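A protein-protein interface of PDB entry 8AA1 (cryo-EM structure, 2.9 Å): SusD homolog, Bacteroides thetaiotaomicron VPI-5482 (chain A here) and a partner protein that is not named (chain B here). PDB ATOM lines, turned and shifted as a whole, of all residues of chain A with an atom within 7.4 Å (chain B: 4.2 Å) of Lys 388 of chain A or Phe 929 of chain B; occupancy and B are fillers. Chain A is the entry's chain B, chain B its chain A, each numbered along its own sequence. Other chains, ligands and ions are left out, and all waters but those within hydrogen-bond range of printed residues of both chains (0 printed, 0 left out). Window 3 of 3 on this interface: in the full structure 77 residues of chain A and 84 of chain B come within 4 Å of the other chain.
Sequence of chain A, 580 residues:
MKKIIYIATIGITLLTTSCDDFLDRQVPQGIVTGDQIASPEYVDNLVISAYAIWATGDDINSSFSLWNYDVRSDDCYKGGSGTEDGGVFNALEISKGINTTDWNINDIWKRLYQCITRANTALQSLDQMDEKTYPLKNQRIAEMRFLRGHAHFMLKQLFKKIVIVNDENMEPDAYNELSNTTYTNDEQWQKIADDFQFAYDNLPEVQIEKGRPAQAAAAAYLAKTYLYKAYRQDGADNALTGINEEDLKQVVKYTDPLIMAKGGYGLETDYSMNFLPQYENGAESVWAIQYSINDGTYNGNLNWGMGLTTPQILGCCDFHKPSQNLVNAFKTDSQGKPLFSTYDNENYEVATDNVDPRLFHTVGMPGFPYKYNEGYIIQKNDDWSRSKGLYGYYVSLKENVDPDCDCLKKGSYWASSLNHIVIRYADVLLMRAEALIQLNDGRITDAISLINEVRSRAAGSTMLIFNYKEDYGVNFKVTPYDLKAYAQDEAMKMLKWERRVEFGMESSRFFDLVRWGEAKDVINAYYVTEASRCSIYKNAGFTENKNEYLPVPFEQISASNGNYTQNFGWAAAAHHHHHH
The side-chain hydroxyl (OG) of Ser 81 of chain A lies within hydrogen-bond range of the backbone NH (N) of Gly 928 of chain B (3.5 Å).
The backbone NH (N) of Gly 428 of chain B sits at hydrogen-bond distance from the side-chain carboxylate (OD2) of Asp 382 of chain A (3.2 Å).
The backbone carbonyl oxygen of Gly 428 of chain B sits at hydrogen-bond distance from the side-chain amino group of Lys 388 of chain A (2.8 Å).
OG of Ser 385 of chain A sits at hydrogen-bond distance from N of Lys 388 of chain A (3.5 Å).
The backbone carbonyl oxygen of Phe 929 of chain B lies within hydrogen-bond range of the side-chain hydroxyl of Tyr 262 of chain B (2.7 Å).
The side-chain amide oxygen (OD1) of Asn 280 of chain B lies within hydrogen-bond range of the backbone NH (N) of Leu 282 of chain B (2.8 Å).
Among the printed residues, pairs that only touch across the chains: Lys 388 of chain A with Phe 929 of chain B (3.3 Å), Lys 388 of chain A with Asn 280 of chain B (3.4 Å) and Lys 388 of chain A with Leu 282 of chain B (3.9 Å).
Of chain B, only Asn 280 (3.4 Å), Leu 282 (3.9 Å), Gly 428 (2.8 Å) and Phe 929 (3.3 Å) come within 4 Å of Lys 388 of chain A.
Phe 929 of chain B touches just one residue of chain A: Lys 388 (3.3 Å).
Printed residues of chain A within 4 Å of Gly 928 of chain B: Ser 81 (3.5 Å).
Of the printed residues of chain A, Leu 282 of chain B touches Lys 388.
Of the printed residues of chain A, Gly 428 of chain B touches Asp 382 (3.2 Å) and Lys 388 (2.8 Å).
Printed residues of chain A within 4 Å of Asn 280 of chain B: Lys 388 (3.4 Å).
Gly 389 of chain A touches none of the printed residues of chain B.
Gly 392 of chain A touches none of the printed residues of chain B.
The nearest residue of chain A that does not touch Phe 929 of chain B is Ser 81 of chain A (5.8 Å).
The nearest printed residue of chain A that does not touch Leu 282 of chain B is Asp 382 of chain A (5.6 Å).
Of the 12 printed residues of chain B, 5 touch a printed residue of chain A.
Printed residues of chain B that touch a printed residue of chain A: Asn 280, Leu 282, Gly 428, Gly 928 and Phe 929.
Hydrophobic or aromatic side chains of chain B within 4 Å of the printed part of chain A: Leu 282 and Phe 929.
Printed residues of chain A that touch a printed residue of chain B: Ser 81, Asp 382 and Lys 388.
Among the printed residues, 6 pairs touch across the chains.
Among the printed residues, no Asp or Glu carboxylate lies within 4 Å of a Lys or Arg side-chain nitrogen of the other chain.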
ATOM      1  N   GLY A  80     -27.781 -23.643   2.658  1.00  0.00           N
ATOM      2  CA  GLY A  80     -27.375 -22.297   3.007  1.00  0.00           C
ATOM      3  C   GLY A  80     -26.060 -22.255   3.758  1.00  0.00           C
ATOM      4  O   GLY A  80     -25.385 -23.264   3.979  1.00  0.00           O
ATOM      5  N   SER A  81     -25.691 -21.035   4.154  1.00  0.00           N
ATOM      6  CA  SER A  81     -24.434 -20.832   4.865  1.00  0.00           C
ATOM      7  C   SER A  81     -24.445 -21.520   6.225  1.00  0.00           C
ATOM      8  O   SER A  81     -23.430 -22.082   6.650  1.00  0.00           O
ATOM      9  CB  SER A  81     -24.157 -19.338   5.022  1.00  0.00           C
ATOM     10  OG  SER A  81     -25.193 -18.705   5.752  1.00  0.00           O
ATOM     11  N   ASP A 318     -26.903 -22.911  -2.127  1.00  0.00           N
ATOM     12  CA  ASP A 318     -26.677 -24.317  -1.781  1.00  0.00           C
ATOM     13  C   ASP A 318     -27.770 -24.957  -0.922  1.00  0.00           C
ATOM     14  O   ASP A 318     -27.458 -25.623   0.070  1.00  0.00           O
ATOM     15  CB  ASP A 318     -25.330 -24.461  -1.069  1.00  0.00           C
ATOM     16  CG  ASP A 318     -24.789 -25.877  -1.127  1.00  0.00           C
ATOM     17  OD1 ASP A 318     -25.349 -26.699  -1.882  1.00  0.00           O
ATOM     18  OD2 ASP A 318     -23.812 -26.169  -0.408  1.00  0.00           O
ATOM     19  N   ASN A 381     -15.288 -29.642  -1.400  1.00  0.00           N
ATOM     20  CA  ASN A 381     -14.598 -28.372  -1.229  1.00  0.00           C
ATOM     21  C   ASN A 381     -15.629 -27.253  -1.174  1.00  0.00           C
ATOM     22  O   ASN A 381     -16.840 -27.492  -1.210  1.00  0.00           O
ATOM     23  CB  ASN A 381     -13.580 -28.140  -2.352  1.00  0.00           C
ATOM     24  CG  ASN A 381     -14.141 -28.459  -3.723  1.00  0.00           C
ATOM     25  OD1 ASN A 381     -15.351 -28.603  -3.894  1.00  0.00           O
ATOM     26  ND2 ASN A 381     -13.260 -28.572  -4.710  1.00  0.00           N
ATOM     27  N   ASP A 382     -15.138 -26.015  -1.086  1.00  0.00           N
ATOM     28  CA  ASP A 382     -16.017 -24.855  -1.014  1.00  0.00           C
ATOM     29  C   ASP A 382     -16.732 -24.570  -2.327  1.00  0.00           C
ATOM     30  O   ASP A 382     -17.701 -23.804  -2.329  1.00  0.00           O
ATOM     31  CB  ASP A 382     -15.223 -23.622  -0.582  1.00  0.00           C
ATOM     32  CG  ASP A 382     -14.622 -23.771   0.801  1.00  0.00           C
ATOM     33  OD1 ASP A 382     -14.827 -24.832   1.428  1.00  0.00           O
ATOM     34  OD2 ASP A 382     -13.943 -22.829   1.260  1.00  0.00           O
ATOM     35  N   SER A 385     -19.999 -26.656  -1.553  1.00  0.00           N
ATOM     36  CA  SER A 385     -20.636 -26.550  -0.249  1.00  0.00           C
ATOM     37  C   SER A 385     -20.549 -25.112   0.235  1.00  0.00           C
ATOM     38  O   SER A 385     -19.482 -24.494   0.170  1.00  0.00           O
ATOM     39  CB  SER A 385     -19.983 -27.491   0.767  1.00  0.00           C
ATOM     40  OG  SER A 385     -20.627 -27.406   2.026  1.00  0.00           O
ATOM     41  N   ARG A 386     -21.672 -24.585   0.719  1.00  0.00           N
ATOM     42  CA  ARG A 386     -21.715 -23.228   1.249  1.00  0.00           C
ATOM     43  C   ARG A 386     -21.534 -23.187   2.759  1.00  0.00           C
ATOM     44  O   ARG A 386     -21.065 -22.175   3.293  1.00  0.00           O
ATOM     45  CB  ARG A 386     -23.041 -22.561   0.874  1.00  0.00           C
ATOM     46  CG  ARG A 386     -23.074 -21.056   1.059  1.00  0.00           C
ATOM     47  CD  ARG A 386     -24.501 -20.543   0.998  1.00  0.00           C
ATOM     48  NE  ARG A 386     -24.564 -19.092   0.883  1.00  0.00           N
ATOM     49  CZ  ARG A 386     -25.678 -18.381   1.001  1.00  0.00           C
ATOM     50  NH1 ARG A 386     -26.841 -18.957   1.251  1.00  0.00           N
ATOM     51  NH2 ARG A 386     -25.620 -17.059   0.870  1.00  0.00           N
ATOM     52  N   SER A 387     -21.890 -24.264   3.453  1.00  0.00           N
ATOM     53  CA  SER A 387     -21.792 -24.336   4.903  1.00  0.00           C
ATOM     54  C   SER A 387     -20.475 -24.933   5.378  1.00  0.00           C
ATOM     55  O   SER A 387     -20.315 -25.167   6.582  1.00  0.00           O
ATOM     56  CB  SER A 387     -22.962 -25.145   5.468  1.00  0.00           C
ATOM     57  OG  SER A 387     -22.951 -26.470   4.970  1.00  0.00           O
ATOM     58  N   LYS A 388     -19.536 -25.188   4.464  1.00  0.00           N
ATOM     59  CA  LYS A 388     -18.221 -25.735   4.799  1.00  0.00           C
ATOM     60  C   LYS A 388     -18.345 -27.084   5.508  1.00  0.00           C
ATOM     61  O   LYS A 388     -17.718 -27.334   6.538  1.00  0.00           O
ATOM     62  CB  LYS A 388     -17.411 -24.744   5.638  1.00  0.00           C
ATOM     63  CG  LYS A 388     -17.217 -23.390   4.978  1.00  0.00           C
ATOM     64  CD  LYS A 388     -16.506 -22.419   5.904  1.00  0.00           C
ATOM     65  CE  LYS A 388     -16.293 -21.075   5.231  1.00  0.00           C
ATOM     66  NZ  LYS A 388     -17.581 -20.453   4.816  1.00  0.00           N
ATOM     67  N   GLY A 389     -19.171 -27.960   4.939  1.00  0.00           N
ATOM     68  CA  GLY A 389     -19.335 -29.302   5.453  1.00  0.00           C
ATOM     69  C   GLY A 389     -20.334 -29.455   6.578  1.00  0.00           C
ATOM     70  O   GLY A 389     -20.500 -30.571   7.085  1.00  0.00           O
ATOM     71  N   LEU A 390     -20.999 -28.375   6.995  1.00  0.00           N
ATOM     72  CA  LEU A 390     -21.990 -28.486   8.061  1.00  0.00           C
ATOM     73  C   LEU A 390     -23.169 -29.350   7.633  1.00  0.00           C
ATOM     74  O   LEU A 390     -23.671 -30.162   8.419  1.00  0.00           O
ATOM     75  CB  LEU A 390     -22.467 -27.096   8.482  1.00  0.00           C
ATOM     76  CG  LEU A 390     -23.545 -27.049   9.565  1.00  0.00           C
ATOM     77  CD1 LEU A 390     -23.052 -27.709  10.842  1.00  0.00           C
ATOM     78  CD2 LEU A 390     -23.976 -25.617   9.832  1.00  0.00           C
ATOM     79  N   TYR A 391     -23.625 -29.193   6.391  1.00  0.00           N
ATOM     80  CA  TYR A 391     -24.753 -29.949   5.863  1.00  0.00           C
ATOM     81  C   TYR A 391     -24.316 -30.986   4.832  1.00  0.00           C
ATOM     82  O   TYR A 391     -25.103 -31.383   3.971  1.00  0.00           O
ATOM     83  CB  TYR A 391     -25.795 -29.008   5.260  1.00  0.00           C
ATOM     84  CG  TYR A 391     -26.386 -28.033   6.251  1.00  0.00           C
ATOM     85  CD1 TYR A 391     -27.247 -28.466   7.250  1.00  0.00           C
ATOM     86  CD2 TYR A 391     -26.092 -26.679   6.182  1.00  0.00           C
ATOM     87  CE1 TYR A 391     -27.792 -27.580   8.155  1.00  0.00           C
ATOM     88  CE2 TYR A 391     -26.633 -25.785   7.085  1.00  0.00           C
ATOM     89  CZ  TYR A 391     -27.483 -26.241   8.069  1.00  0.00           C
ATOM     90  OH  TYR A 391     -28.026 -25.356   8.970  1.00  0.00           O
ATOM     91  N   GLY A 392     -23.067 -31.430   4.907  1.00  0.00           N
ATOM     92  CA  GLY A 392     -22.567 -32.414   3.974  1.00  0.00           C
ATOM     93  C   GLY A 392     -22.206 -31.809   2.630  1.00  0.00           C
ATOM     94  O   GLY A 392     -22.145 -30.589   2.448  1.00  0.00           O
ATOM     95  N   TYR A 393     -21.962 -32.699   1.666  1.00  0.00           N
ATOM     96  CA  TYR A 393     -21.573 -32.294   0.320  1.00  0.00           C
ATOM     97  C   TYR A 393     -22.470 -32.915  -0.746  1.00  0.00           C
ATOM     98  O   TYR A 393     -22.089 -32.958  -1.919  1.00  0.00           O
ATOM     99  CB  TYR A 393     -20.110 -32.651   0.051  1.00  0.00           C
ATOM    100  CG  TYR A 393     -19.140 -32.000   1.010  1.00  0.00           C
ATOM    101  CD1 TYR A 393     -18.605 -30.748   0.742  1.00  0.00           C
ATOM    102  CD2 TYR A 393     -18.759 -32.637   2.184  1.00  0.00           C
ATOM    103  CE1 TYR A 393     -17.719 -30.148   1.615  1.00  0.00           C
ATOM    104  CE2 TYR A 393     -17.874 -32.045   3.062  1.00  0.00           C
ATOM    105  CZ  TYR A 393     -17.357 -30.800   2.773  1.00  0.00           C
ATOM    106  OH  TYR A 393     -16.475 -30.206   3.645  1.00  0.00           O
ATOM    107  N   TYR B 262     -10.681  -9.642  12.657  1.00  0.00           N
ATOM    108  CA  TYR B 262     -11.642 -10.615  12.148  1.00  0.00           C
ATOM    109  C   TYR B 262     -11.183 -12.039  12.431  1.00  0.00           C
ATOM    110  O   TYR B 262     -11.980 -12.885  12.857  1.00  0.00           O
ATOM    111  CB  TYR B 262     -11.849 -10.400  10.647  1.00  0.00           C
ATOM    112  CG  TYR B 262     -12.804 -11.372   9.995  1.00  0.00           C
ATOM    113  CD1 TYR B 262     -14.175 -11.164  10.039  1.00  0.00           C
ATOM    114  CD2 TYR B 262     -12.333 -12.491   9.323  1.00  0.00           C
ATOM    115  CE1 TYR B 262     -15.050 -12.046   9.439  1.00  0.00           C
ATOM    116  CE2 TYR B 262     -13.200 -13.379   8.721  1.00  0.00           C
ATOM    117  CZ  TYR B 262     -14.557 -13.151   8.782  1.00  0.00           C
ATOM    118  OH  TYR B 262     -15.423 -14.034   8.183  1.00  0.00           O
ATOM    119  N   MET B 266     -13.114 -14.729  14.842  1.00  0.00           N
ATOM    120  CA  MET B 266     -13.513 -16.046  14.353  1.00  0.00           C
ATOM    121  C   MET B 266     -12.908 -17.154  15.206  1.00  0.00           C
ATOM    122  O   MET B 266     -13.581 -18.145  15.520  1.00  0.00           O
ATOM    123  CB  MET B 266     -13.114 -16.206  12.887  1.00  0.00           C
ATOM    124  CG  MET B 266     -13.278 -17.617  12.353  1.00  0.00           C
ATOM    125  SD  MET B 266     -13.301 -17.682  10.552  1.00  0.00           S
ATOM    126  CE  MET B 266     -11.634 -17.153  10.176  1.00  0.00           C
ATOM    127  N   TYR B 270     -14.950 -19.934  17.379  1.00  0.00           N
ATOM    128  CA  TYR B 270     -14.709 -21.361  17.198  1.00  0.00           C
ATOM    129  C   TYR B 270     -14.353 -22.041  18.514  1.00  0.00           C
ATOM    130  O   TYR B 270     -14.848 -23.134  18.808  1.00  0.00           O
ATOM    131  CB  TYR B 270     -13.600 -21.580  16.168  1.00  0.00           C
ATOM    132  CG  TYR B 270     -14.105 -21.816  14.764  1.00  0.00           C
ATOM    133  CD1 TYR B 270     -14.580 -23.063  14.379  1.00  0.00           C
ATOM    134  CD2 TYR B 270     -14.102 -20.798  13.822  1.00  0.00           C
ATOM    135  CE1 TYR B 270     -15.041 -23.285  13.096  1.00  0.00           C
ATOM    136  CE2 TYR B 270     -14.560 -21.010  12.537  1.00  0.00           C
ATOM    137  CZ  TYR B 270     -15.029 -22.256  12.180  1.00  0.00           C
ATOM    138  OH  TYR B 270     -15.486 -22.473  10.901  1.00  0.00           O
ATOM    139  N   ASN B 280     -11.717 -23.484   9.768  1.00  0.00           N
ATOM    140  CA  ASN B 280     -12.470 -22.341   9.261  1.00  0.00           C
ATOM    141  C   ASN B 280     -12.505 -22.313   7.738  1.00  0.00           C
ATOM    142  O   ASN B 280     -13.437 -21.747   7.155  1.00  0.00           O
ATOM    143  CB  ASN B 280     -11.874 -21.041   9.799  1.00  0.00           C
ATOM    144  CG  ASN B 280     -10.419 -20.865   9.416  1.00  0.00           C
ATOM    145  OD1 ASN B 280     -10.105 -20.297   8.371  1.00  0.00           O
ATOM    146  ND2 ASN B 280      -9.522 -21.356  10.262  1.00  0.00           N
ATOM    147  N   LEU B 282     -10.831 -20.613   5.675  1.00  0.00           N
ATOM    148  CA  LEU B 282     -10.724 -19.249   5.174  1.00  0.00           C
ATOM    149  C   LEU B 282      -9.274 -18.788   5.077  1.00  0.00           C
ATOM    150  O   LEU B 282      -9.015 -17.587   4.966  1.00  0.00           O
ATOM    151  CB  LEU B 282     -11.526 -18.286   6.052  1.00  0.00           C
ATOM    152  CG  LEU B 282     -13.048 -18.412   5.989  1.00  0.00           C
ATOM    153  CD1 LEU B 282     -13.702 -17.321   6.818  1.00  0.00           C
ATOM    154  CD2 LEU B 282     -13.533 -18.358   4.550  1.00  0.00           C
ATOM    155  N   GLY B 428     -14.923 -19.957   0.328  1.00  0.00           N
ATOM    156  CA  GLY B 428     -15.884 -19.944   1.410  1.00  0.00           C
ATOM    157  C   GLY B 428     -16.223 -18.583   1.974  1.00  0.00           C
ATOM    158  O   GLY B 428     -16.943 -18.507   2.975  1.00  0.00           O
ATOM    159  N   PRO B 430     -18.097 -15.013   2.493  1.00  0.00           N
ATOM    160  CA  PRO B 430     -19.531 -14.726   2.366  1.00  0.00           C
ATOM    161  C   PRO B 430     -19.851 -13.989   1.074  1.00  0.00           C
ATOM    162  O   PRO B 430     -19.044 -13.218   0.553  1.00  0.00           O
ATOM    163  CB  PRO B 430     -19.829 -13.857   3.592  1.00  0.00           C
ATOM    164  CG  PRO B 430     -18.517 -13.253   3.952  1.00  0.00           C
ATOM    165  CD  PRO B 430     -17.496 -14.302   3.634  1.00  0.00           C
ATOM    166  N   GLY B 928     -23.300 -16.252   7.316  1.00  0.00           N
ATOM    167  CA  GLY B 928     -22.228 -16.233   8.285  1.00  0.00           C
ATOM    168  C   GLY B 928     -20.949 -15.619   7.744  1.00  0.00           C
ATOM    169  O   GLY B 928     -20.836 -15.262   6.572  1.00  0.00           O
ATOM    170  N   PHE B 929     -19.972 -15.494   8.643  1.00  0.00           N
ATOM    171  CA  PHE B 929     -18.634 -14.993   8.336  1.00  0.00           C
ATOM    172  C   PHE B 929     -18.646 -13.566   7.798  1.00  0.00           C
ATOM    173  O   PHE B 929     -17.721 -13.162   7.087  1.00  0.00           O
ATOM    174  CB  PHE B 929     -17.905 -15.921   7.357  1.00  0.00           C
ATOM    175  CG  PHE B 929     -17.687 -17.307   7.889  1.00  0.00           C
ATOM    176  CD1 PHE B 929     -16.670 -17.562   8.793  1.00  0.00           C
ATOM    177  CD2 PHE B 929     -18.495 -18.354   7.484  1.00  0.00           C
ATOM    178  CE1 PHE B 929     -16.466 -18.835   9.285  1.00  0.00           C
ATOM    179  CE2 PHE B 929     -18.295 -19.630   7.972  1.00  0.00           C
ATOM    180  CZ  PHE B 929     -17.279 -19.871   8.874  1.00  0.00           C
ATOM    181  N   LEU B 930     -19.673 -12.790   8.125  1.00  0.00           N
ATOM    182  CA  LEU B 930     -19.709 -11.392   7.733  1.00  0.00           C
ATOM    183  C   LEU B 930     -18.848 -10.552   8.670  1.00  0.00           C
ATOM    184  O   LEU B 930     -18.549 -10.943   9.803  1.00  0.00           O
ATOM    185  CB  LEU B 930     -21.144 -10.866   7.731  1.00  0.00           C
ATOM    186  CG  LEU B 930     -22.049 -11.317   6.586  1.00  0.00           C
ATOM    187  CD1 LEU B 930     -23.422 -10.680   6.718  1.00  0.00           C
ATOM    188  CD2 LEU B 930     -21.424 -10.977   5.245  1.00  0.00           C
ATOM    189  N   ASN B 931     -18.446  -9.382   8.182  1.00  0.00           N
ATOM    190  CA  ASN B 931     -17.667  -8.464   9.000  1.00  0.00           C
ATOM    191  C   ASN B 931     -18.553  -7.833  10.068  1.00  0.00           C
ATOM    192  O   ASN B 931     -19.716  -7.501   9.817  1.00  0.00           O
ATOM    193  CB  ASN B 931     -17.034  -7.383   8.126  1.00  0.00           C
ATOM    194  CG  ASN B 931     -15.901  -6.661   8.822  1.00  0.00           C
ATOM    195  OD1 ASN B 931     -15.359  -7.147   9.814  1.00  0.00           O
ATOM    196  ND2 ASN B 931     -15.533  -5.498   8.302  1.00  0.00           N
ATOM    197  N   ARG B 954     -20.880 -19.465  16.688  1.00  0.00           N
ATOM    198  CA  ARG B 954     -21.191 -19.616  15.275  1.00  0.00           C
ATOM    199  C   ARG B 954     -22.615 -20.090  15.024  1.00  0.00           C
ATOM    200  O   ARG B 954     -23.054 -20.098  13.869  1.00  0.00           O
ATOM    201  CB  ARG B 954     -20.214 -20.592  14.615  1.00  0.00           C
ATOM    202  CG  ARG B 954     -18.755 -20.333  14.942  1.00  0.00           C
ATOM    203  CD  ARG B 954     -17.830 -21.048  13.969  1.00  0.00           C
ATOM    204  NE  ARG B 954     -18.169 -22.457  13.811  1.00  0.00           N
ATOM    205  CZ  ARG B 954     -18.734 -22.977  12.730  1.00  0.00           C
ATOM    206  NH1 ARG B 954     -19.041 -22.227  11.683  1.00  0.00           N
ATOM    207  NH2 ARG B 954     -18.998 -24.279  12.696  1.00  0.00           N
